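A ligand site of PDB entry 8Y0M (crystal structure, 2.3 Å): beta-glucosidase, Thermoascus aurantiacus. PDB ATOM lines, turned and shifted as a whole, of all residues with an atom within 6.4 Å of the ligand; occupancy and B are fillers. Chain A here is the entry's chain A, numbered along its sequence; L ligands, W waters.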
ATOM      1  N   TRP A  69       9.736 -20.822 -25.666  1.00  0.00           N
ATOM      2  CA  TRP A  69       9.108 -20.657 -26.966  1.00  0.00           C
ATOM      3  C   TRP A  69       9.016 -22.002 -27.680  1.00  0.00           C
ATOM      4  O   TRP A  69      10.033 -22.635 -27.928  1.00  0.00           O
ATOM      5  CB  TRP A  69       9.913 -19.642 -27.797  1.00  0.00           C
ATOM      6  CG  TRP A  69       9.374 -19.388 -29.184  1.00  0.00           C
ATOM      7  CD1 TRP A  69      10.091 -19.451 -30.347  1.00  0.00           C
ATOM      8  CD2 TRP A  69       8.042 -18.980 -29.560  1.00  0.00           C
ATOM      9  NE1 TRP A  69       9.294 -19.149 -31.409  1.00  0.00           N
ATOM     10  CE2 TRP A  69       8.035 -18.848 -30.963  1.00  0.00           C
ATOM     11  CE3 TRP A  69       6.858 -18.727 -28.856  1.00  0.00           C
ATOM     12  CZ2 TRP A  69       6.889 -18.481 -31.678  1.00  0.00           C
ATOM     13  CZ3 TRP A  69       5.731 -18.358 -29.559  1.00  0.00           C
ATOM     14  CH2 TRP A  69       5.750 -18.234 -30.943  1.00  0.00           C
ATOM     15  N   VAL A  75       0.748 -21.219 -27.297  1.00  0.00           N
ATOM     16  CA  VAL A  75       1.616 -20.114 -27.670  1.00  0.00           C
ATOM     17  C   VAL A  75       2.459 -19.722 -26.462  1.00  0.00           C
ATOM     18  O   VAL A  75       3.610 -19.320 -26.608  1.00  0.00           O
ATOM     19  CB  VAL A  75       0.799 -18.933 -28.246  1.00  0.00           C
ATOM     20  CG1 VAL A  75       1.630 -17.662 -28.368  1.00  0.00           C
ATOM     21  CG2 VAL A  75       0.178 -19.303 -29.579  1.00  0.00           C
ATOM     22  N   ASP A  93      -3.294 -17.174 -28.508  1.00  0.00           N
ATOM     23  CA  ASP A  93      -3.880 -16.167 -29.385  1.00  0.00           C
ATOM     24  C   ASP A  93      -5.183 -16.721 -29.937  1.00  0.00           C
ATOM     25  O   ASP A  93      -5.354 -17.936 -29.963  1.00  0.00           O
ATOM     26  CB  ASP A  93      -2.888 -15.770 -30.479  1.00  0.00           C
ATOM     27  CG  ASP A  93      -1.625 -15.062 -30.027  1.00  0.00           C
ATOM     28  OD1 ASP A  93      -1.740 -14.091 -29.244  1.00  0.00           O
ATOM     29  OD2 ASP A  93      -0.538 -15.453 -30.487  1.00  0.00           O
ATOM     30  N   PRO A  95      -7.239 -12.358 -30.531  1.00  0.00           N
ATOM     31  CA  PRO A  95      -8.468 -11.599 -30.277  1.00  0.00           C
ATOM     32  C   PRO A  95      -9.698 -11.896 -31.126  1.00  0.00           C
ATOM     33  O   PRO A  95     -10.774 -11.403 -30.810  1.00  0.00           O
ATOM     34  CB  PRO A  95      -7.984 -10.151 -30.508  1.00  0.00           C
ATOM     35  CG  PRO A  95      -6.494 -10.208 -30.255  1.00  0.00           C
ATOM     36  CD  PRO A  95      -6.119 -11.498 -30.950  1.00  0.00           C
ATOM     37  N   ARG A  99      -5.939 -19.262 -32.500  1.00  0.00           N
ATOM     38  CA  ARG A  99      -4.853 -19.303 -33.467  1.00  0.00           C
ATOM     39  C   ARG A  99      -4.200 -20.678 -33.430  1.00  0.00           C
ATOM     40  O   ARG A  99      -4.251 -21.369 -32.421  1.00  0.00           O
ATOM     41  CB  ARG A  99      -3.844 -18.197 -33.127  1.00  0.00           C
ATOM     42  CG  ARG A  99      -2.771 -17.988 -34.172  1.00  0.00           C
ATOM     43  CD  ARG A  99      -1.753 -16.996 -33.641  1.00  0.00           C
ATOM     44  NE  ARG A  99      -0.644 -16.767 -34.578  1.00  0.00           N
ATOM     45  CZ  ARG A  99       0.533 -16.266 -34.243  1.00  0.00           C
ATOM     46  NH1 ARG A  99       0.823 -15.961 -32.990  1.00  0.00           N
ATOM     47  NH2 ARG A  99       1.451 -16.091 -35.182  1.00  0.00           N
ATOM     48  N   PHE A 100      -3.617 -21.067 -34.579  1.00  0.00           N
ATOM     49  CA  PHE A 100      -2.781 -22.255 -34.697  1.00  0.00           C
ATOM     50  C   PHE A 100      -3.557 -23.514 -34.339  1.00  0.00           C
ATOM     51  O   PHE A 100      -2.989 -24.465 -33.802  1.00  0.00           O
ATOM     52  CB  PHE A 100      -1.545 -22.187 -33.789  1.00  0.00           C
ATOM     53  CG  PHE A 100      -0.490 -21.169 -34.186  1.00  0.00           C
ATOM     54  CD1 PHE A 100      -0.170 -20.941 -35.517  1.00  0.00           C
ATOM     55  CD2 PHE A 100       0.203 -20.459 -33.205  1.00  0.00           C
ATOM     56  CE1 PHE A 100       0.802 -20.023 -35.867  1.00  0.00           C
ATOM     57  CE2 PHE A 100       1.184 -19.539 -33.559  1.00  0.00           C
ATOM     58  CZ  PHE A 100       1.484 -19.326 -34.891  1.00  0.00           C
ATOM     59  N   LEU A 142      -5.592 -14.579 -25.503  1.00  0.00           N
ATOM     60  CA  LEU A 142      -4.753 -13.394 -25.538  1.00  0.00           C
ATOM     61  C   LEU A 142      -5.448 -12.300 -26.344  1.00  0.00           C
ATOM     62  O   LEU A 142      -5.094 -12.005 -27.483  1.00  0.00           O
ATOM     63  CB  LEU A 142      -3.363 -13.729 -26.090  1.00  0.00           C
ATOM     64  CG  LEU A 142      -2.585 -14.783 -25.285  1.00  0.00           C
ATOM     65  CD1 LEU A 142      -1.303 -15.157 -25.996  1.00  0.00           C
ATOM     66  CD2 LEU A 142      -2.289 -14.295 -23.878  1.00  0.00           C
ATOM     67  N   VAL A 145      -8.232  -6.342 -27.556  1.00  0.00           N
ATOM     68  CA  VAL A 145      -7.237  -5.303 -27.739  1.00  0.00           C
ATOM     69  C   VAL A 145      -7.865  -3.924 -27.590  1.00  0.00           C
ATOM     70  O   VAL A 145      -8.849  -3.622 -28.255  1.00  0.00           O
ATOM     71  CB  VAL A 145      -6.553  -5.439 -29.118  1.00  0.00           C
ATOM     72  CG1 VAL A 145      -5.587  -4.288 -29.386  1.00  0.00           C
ATOM     73  CG2 VAL A 145      -5.862  -6.780 -29.281  1.00  0.00           C
ATOM     74  N   ARG A 157      -1.676  -2.492 -36.486  1.00  0.00           N
ATOM     75  CA  ARG A 157      -2.461  -3.432 -35.701  1.00  0.00           C
ATOM     76  C   ARG A 157      -3.757  -2.810 -35.174  1.00  0.00           C
ATOM     77  O   ARG A 157      -4.416  -3.426 -34.339  1.00  0.00           O
ATOM     78  CB  ARG A 157      -1.647  -3.931 -34.502  1.00  0.00           C
ATOM     79  CG  ARG A 157      -0.390  -4.704 -34.879  1.00  0.00           C
ATOM     80  CD  ARG A 157       0.272  -5.308 -33.649  1.00  0.00           C
ATOM     81  NE  ARG A 157      -0.490  -6.447 -33.119  1.00  0.00           N
ATOM     82  CZ  ARG A 157      -0.120  -7.217 -32.102  1.00  0.00           C
ATOM     83  NH1 ARG A 157       0.982  -6.952 -31.422  1.00  0.00           N
ATOM     84  NH2 ARG A 157      -0.865  -8.255 -31.768  1.00  0.00           N
ATOM     85  N   GLU A 160      -7.056  -4.874 -34.987  1.00  0.00           N
ATOM     86  CA  GLU A 160      -7.226  -5.880 -33.949  1.00  0.00           C
ATOM     87  C   GLU A 160      -8.050  -5.319 -32.799  1.00  0.00           C
ATOM     88  O   GLU A 160      -8.737  -6.063 -32.104  1.00  0.00           O
ATOM     89  CB  GLU A 160      -5.882  -6.334 -33.359  1.00  0.00           C
ATOM     90  CG  GLU A 160      -5.015  -7.148 -34.320  1.00  0.00           C
ATOM     91  CD  GLU A 160      -3.998  -7.996 -33.587  1.00  0.00           C
ATOM     92  OE1 GLU A 160      -4.424  -8.800 -32.737  1.00  0.00           O
ATOM     93  OE2 GLU A 160      -2.780  -7.859 -33.853  1.00  0.00           O
ATOM     94  N   LYS A 190      -4.898  -6.332 -23.807  1.00  0.00           N
ATOM     95  CA  LYS A 190      -3.589  -6.008 -24.359  1.00  0.00           C
ATOM     96  C   LYS A 190      -3.750  -4.868 -25.364  1.00  0.00           C
ATOM     97  O   LYS A 190      -4.867  -4.623 -25.819  1.00  0.00           O
ATOM     98  CB  LYS A 190      -2.974  -7.261 -25.001  1.00  0.00           C
ATOM     99  CG  LYS A 190      -3.497  -7.651 -26.383  1.00  0.00           C
ATOM    100  CD  LYS A 190      -2.952  -8.990 -26.867  1.00  0.00           C
ATOM    101  CE  LYS A 190      -3.335  -9.355 -28.265  1.00  0.00           C
ATOM    102  NZ  LYS A 190      -2.856 -10.704 -28.602  1.00  0.00           N
ATOM    103  N   HIS A 191      -2.672  -4.154 -25.715  1.00  0.00           N
ATOM    104  CA  HIS A 191      -1.354  -4.215 -25.085  1.00  0.00           C
ATOM    105  C   HIS A 191      -1.188  -2.946 -24.254  1.00  0.00           C
ATOM    106  O   HIS A 191      -1.434  -1.845 -24.738  1.00  0.00           O
ATOM    107  CB  HIS A 191      -0.254  -4.266 -26.154  1.00  0.00           C
ATOM    108  CG  HIS A 191      -0.444  -5.340 -27.175  1.00  0.00           C
ATOM    109  ND1 HIS A 191      -1.274  -5.176 -28.268  1.00  0.00           N
ATOM    110  CD2 HIS A 191       0.056  -6.580 -27.276  1.00  0.00           C
ATOM    111  CE1 HIS A 191      -1.252  -6.282 -28.998  1.00  0.00           C
ATOM    112  NE2 HIS A 191      -0.453  -7.146 -28.413  1.00  0.00           N
ATOM    113  N   ASN A 195       1.378   1.214 -27.311  1.00  0.00           N
ATOM    114  CA  ASN A 195       1.898   0.486 -28.454  1.00  0.00           C
ATOM    115  C   ASN A 195       1.103   0.862 -29.691  1.00  0.00           C
ATOM    116  O   ASN A 195       0.392   0.034 -30.266  1.00  0.00           O
ATOM    117  CB  ASN A 195       1.874  -1.017 -28.180  1.00  0.00           C
ATOM    118  CG  ASN A 195       2.576  -1.829 -29.250  1.00  0.00           C
ATOM    119  OD1 ASN A 195       3.320  -1.290 -30.070  1.00  0.00           O
ATOM    120  ND2 ASN A 195       2.363  -3.143 -29.241  1.00  0.00           N
ATOM    121  N   GLU A 198       3.888  -0.202 -34.985  1.00  0.00           N
ATOM    122  CA  GLU A 198       4.754  -1.364 -35.039  1.00  0.00           C
ATOM    123  C   GLU A 198       6.221  -0.957 -35.144  1.00  0.00           C
ATOM    124  O   GLU A 198       7.090  -1.690 -34.670  1.00  0.00           O
ATOM    125  CB  GLU A 198       4.345  -2.279 -36.190  1.00  0.00           C
ATOM    126  CG  GLU A 198       3.004  -2.964 -35.935  1.00  0.00           C
ATOM    127  CD  GLU A 198       2.979  -3.715 -34.614  1.00  0.00           C
ATOM    128  OE1 GLU A 198       3.555  -4.829 -34.558  1.00  0.00           O
ATOM    129  OE2 GLU A 198       2.421  -3.174 -33.641  1.00  0.00           O
ATOM    130  N   ARG A 201       9.095  -1.319 -32.263  1.00  0.00           N
ATOM    131  CA  ARG A 201       8.437  -1.842 -31.073  1.00  0.00           C
ATOM    132  C   ARG A 201       9.418  -2.717 -30.295  1.00  0.00           C
ATOM    133  O   ARG A 201       9.318  -2.822 -29.073  1.00  0.00           O
ATOM    134  CB  ARG A 201       7.167  -2.623 -31.418  1.00  0.00           C
ATOM    135  CG  ARG A 201       7.378  -3.982 -32.061  1.00  0.00           C
ATOM    136  CD  ARG A 201       6.067  -4.520 -32.596  1.00  0.00           C
ATOM    137  NE  ARG A 201       6.261  -5.837 -33.203  1.00  0.00           N
ATOM    138  CZ  ARG A 201       5.572  -6.947 -32.918  1.00  0.00           C
ATOM    139  NH1 ARG A 201       4.543  -6.911 -32.081  1.00  0.00           N
ATOM    140  NH2 ARG A 201       5.897  -8.080 -33.506  1.00  0.00           N
ATOM    141  N   MET A 246      -1.715  -7.704 -20.466  1.00  0.00           N
ATOM    142  CA  MET A 246      -0.423  -7.923 -21.094  1.00  0.00           C
ATOM    143  C   MET A 246       0.282  -6.590 -21.266  1.00  0.00           C
ATOM    144  O   MET A 246      -0.207  -5.723 -21.983  1.00  0.00           O
ATOM    145  CB  MET A 246      -0.559  -8.587 -22.477  1.00  0.00           C
ATOM    146  CG  MET A 246       0.771  -8.849 -23.166  1.00  0.00           C
ATOM    147  SD  MET A 246       0.624  -9.460 -24.858  1.00  0.00           S
ATOM    148  CE  MET A 246      -0.253 -11.008 -24.588  1.00  0.00           C
ATOM    149  N   TYR A 249       5.466  -4.142 -25.581  1.00  0.00           N
ATOM    150  CA  TYR A 249       6.864  -4.196 -26.000  1.00  0.00           C
ATOM    151  C   TYR A 249       7.549  -2.840 -25.852  1.00  0.00           C
ATOM    152  O   TYR A 249       8.744  -2.790 -25.542  1.00  0.00           O
ATOM    153  CB  TYR A 249       6.992  -4.592 -27.479  1.00  0.00           C
ATOM    154  CG  TYR A 249       6.871  -6.080 -27.779  1.00  0.00           C
ATOM    155  CD1 TYR A 249       7.684  -7.011 -27.146  1.00  0.00           C
ATOM    156  CD2 TYR A 249       5.938  -6.554 -28.699  1.00  0.00           C
ATOM    157  CE1 TYR A 249       7.574  -8.366 -27.414  1.00  0.00           C
ATOM    158  CE2 TYR A 249       5.822  -7.909 -28.975  1.00  0.00           C
ATOM    159  CZ  TYR A 249       6.645  -8.818 -28.335  1.00  0.00           C
ATOM    160  OH  TYR A 249       6.525 -10.142 -28.620  1.00  0.00           O
ATOM    161  N   ASP A 281       4.276  -9.300 -22.771  1.00  0.00           N
ATOM    162  CA  ASP A 281       4.286  -9.685 -24.176  1.00  0.00           C
ATOM    163  C   ASP A 281       5.526 -10.552 -24.393  1.00  0.00           C
ATOM    164  O   ASP A 281       6.441 -10.555 -23.571  1.00  0.00           O
ATOM    165  CB  ASP A 281       4.155  -8.498 -25.105  1.00  0.00           C
ATOM    166  CG  ASP A 281       3.573  -8.831 -26.473  1.00  0.00           C
ATOM    167  OD1 ASP A 281       3.526 -10.034 -26.810  1.00  0.00           O
ATOM    168  OD2 ASP A 281       3.135  -7.892 -27.184  1.00  0.00           O
ATOM    169  N   TRP A 282       5.519 -11.320 -25.482  1.00  0.00           N
ATOM    170  CA  TRP A 282       6.454 -12.409 -25.683  1.00  0.00           C
ATOM    171  C   TRP A 282       7.861 -11.875 -25.936  1.00  0.00           C
ATOM    172  O   TRP A 282       8.149 -11.356 -27.015  1.00  0.00           O
ATOM    173  CB  TRP A 282       5.990 -13.305 -26.835  1.00  0.00           C
ATOM    174  CG  TRP A 282       5.124 -14.468 -26.429  1.00  0.00           C
ATOM    175  CD1 TRP A 282       5.229 -15.747 -26.899  1.00  0.00           C
ATOM    176  CD2 TRP A 282       4.017 -14.467 -25.499  1.00  0.00           C
ATOM    177  NE1 TRP A 282       4.276 -16.546 -26.311  1.00  0.00           N
ATOM    178  CE2 TRP A 282       3.517 -15.790 -25.466  1.00  0.00           C
ATOM    179  CE3 TRP A 282       3.395 -13.492 -24.708  1.00  0.00           C
ATOM    180  CZ2 TRP A 282       2.433 -16.156 -24.666  1.00  0.00           C
ATOM    181  CZ3 TRP A 282       2.322 -13.866 -23.915  1.00  0.00           C
ATOM    182  CH2 TRP A 282       1.859 -15.178 -23.893  1.00  0.00           C
ATOM    183  N   SER A 451      -0.094 -12.104 -35.209  1.00  0.00           N
ATOM    184  CA  SER A 451      -0.565 -12.948 -34.132  1.00  0.00           C
ATOM    185  C   SER A 451      -2.074 -12.860 -33.997  1.00  0.00           C
ATOM    186  O   SER A 451      -2.698 -13.771 -33.451  1.00  0.00           O
ATOM    187  CB  SER A 451       0.108 -12.571 -32.831  1.00  0.00           C
ATOM    188  OG  SER A 451      -0.223 -11.247 -32.445  1.00  0.00           O
ATOM    189  N   GLY A 452      -2.666 -11.765 -34.491  1.00  0.00           N
ATOM    190  CA  GLY A 452      -4.071 -11.498 -34.285  1.00  0.00           C
ATOM    191  C   GLY A 452      -4.970 -12.268 -35.258  1.00  0.00           C
ATOM    192  O   GLY A 452      -5.911 -11.696 -35.800  1.00  0.00           O
ATOM    193  N   GLU A 510       0.934  -7.114 -37.877  1.00  0.00           N
ATOM    194  CA  GLU A 510       1.978  -7.065 -36.874  1.00  0.00           C
ATOM    195  C   GLU A 510       3.330  -6.895 -37.564  1.00  0.00           C
ATOM    196  O   GLU A 510       3.521  -7.304 -38.706  1.00  0.00           O
ATOM    197  CB  GLU A 510       1.897  -8.331 -36.017  1.00  0.00           C
ATOM    198  CG  GLU A 510       2.753  -8.237 -34.756  1.00  0.00           C
ATOM    199  CD  GLU A 510       2.604  -9.402 -33.794  1.00  0.00           C
ATOM    200  OE1 GLU A 510       3.493  -9.552 -32.937  1.00  0.00           O
ATOM    201  OE2 GLU A 510       1.601 -10.133 -33.891  1.00  0.00           O
HETATM  202  C1  LIG L   1       3.361 -10.741 -29.752  1.00  0.00           C
HETATM  203  C2  LIG L   1       2.074  -9.933 -29.908  1.00  0.00           C
HETATM  204  O1  LIG L   1       2.400  -8.556 -29.714  1.00  0.00           O
HETATM  205  C3  LIG L   1       0.973 -10.353 -28.946  1.00  0.00           C
HETATM  206  O2  LIG L   1      -0.243  -9.675 -29.279  1.00  0.00           O
HETATM  207  C4  LIG L   1       0.776 -11.848 -29.012  1.00  0.00           C
HETATM  208  O3  LIG L   1      -0.235 -12.231 -28.082  1.00  0.00           O
HETATM  209  C5  LIG L   1       2.070 -12.575 -28.658  1.00  0.00           C
HETATM  210  N1  LIG L   1       3.145 -12.188 -29.581  1.00  0.00           N
HETATM  211  C6  LIG L   1       1.925 -14.097 -28.675  1.00  0.00           C
HETATM  212  O4  LIG L   1       1.885 -14.578 -30.017  1.00  0.00           O
HETATM  213  O   HOH W   1      -2.787 -10.536 -31.345  1.00  0.00           O
HETATM  214  O   HOH W   2       5.495 -13.607 -30.089  1.00  0.00           O
HETATM  215  O   HOH W   3       3.837 -12.269 -32.563  1.00  0.00           O
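Val 75 touches the ligand.
Leu 142 touches the ligand (CD1 to O3, 3.7 Å).
Arg 201 touches the ligand (NH1 to O1, 3.6 Å).
Met 246 touches the ligand.
Tyr 249 touches the ligand (OH to C1, 3.4 Å).
Trp 282 touches the ligand (CD2 to C6, 3.8 Å).
Ser 451 touches the ligand.
OE1 of Glu 510 touches C2 of the ligand (3.4 Å).
Hydrophobic or aromatic side chains within 4 Å of the ligand: Val 75, Leu 142, His 191, Met 246, Tyr 249 and Trp 282.
OG of Ser 451 is in hydrogen-bond range of OE2 of Glu 510.
A ring nitrogen (NE2) of His 191 lies within hydrogen-bond range of the guanidinium group of Arg 157 (3.3 Å).
The side-chain carboxylate (OE2) of Glu 510 is in salt-bridge range of the guanidinium group (NH2) of Arg 157 (3.8 Å).
The side-chain carboxylate (OE1) of Glu 198 is in salt-bridge range of the guanidinium group (NE) of Arg 201 (3.2 Å).
The backbone carbonyl oxygen of Val 75 is in hydrogen-bond range of the indole nitrogen of Trp 282 (2.9 Å).
The side-chain carboxylate of Glu 160 is in salt-bridge range of the guanidinium group of Arg 157, 2.8 Å away.
OD2 of Asp 93 is in salt-bridge range of NH1 of Arg 99, 2.9 Å away.
NH2 of Arg 157 sits at hydrogen-bond distance from OG of Ser 451 (3.1 Å).
The side-chain amino group (NZ) of Lys 190 sits at hydrogen-bond distance from an oxygen (O2) of the ligand (2.9 Å).
NE2 of His 191 sits at hydrogen-bond distance from O2 of the ligand, 2.7 Å away.
O1 of the ligand sits at hydrogen-bond distance from NH1 of Arg 157 (2.7 Å).
An oxygen (O4) of the ligand sits at hydrogen-bond distance from the guanidinium group (NH1) of Arg 99 (3.4 Å).
O4 of the ligand lies within hydrogen-bond range of OD2 of Asp 93, 2.6 Å away.
The side-chain carboxylate of Asp 281 lies within salt-bridge range of a nitrogen (N1) of the ligand (3.5 Å).
Water W3 bridges OE1 of Glu 510 (2.8 Å) and N1 of the ligand (3.1 Å).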
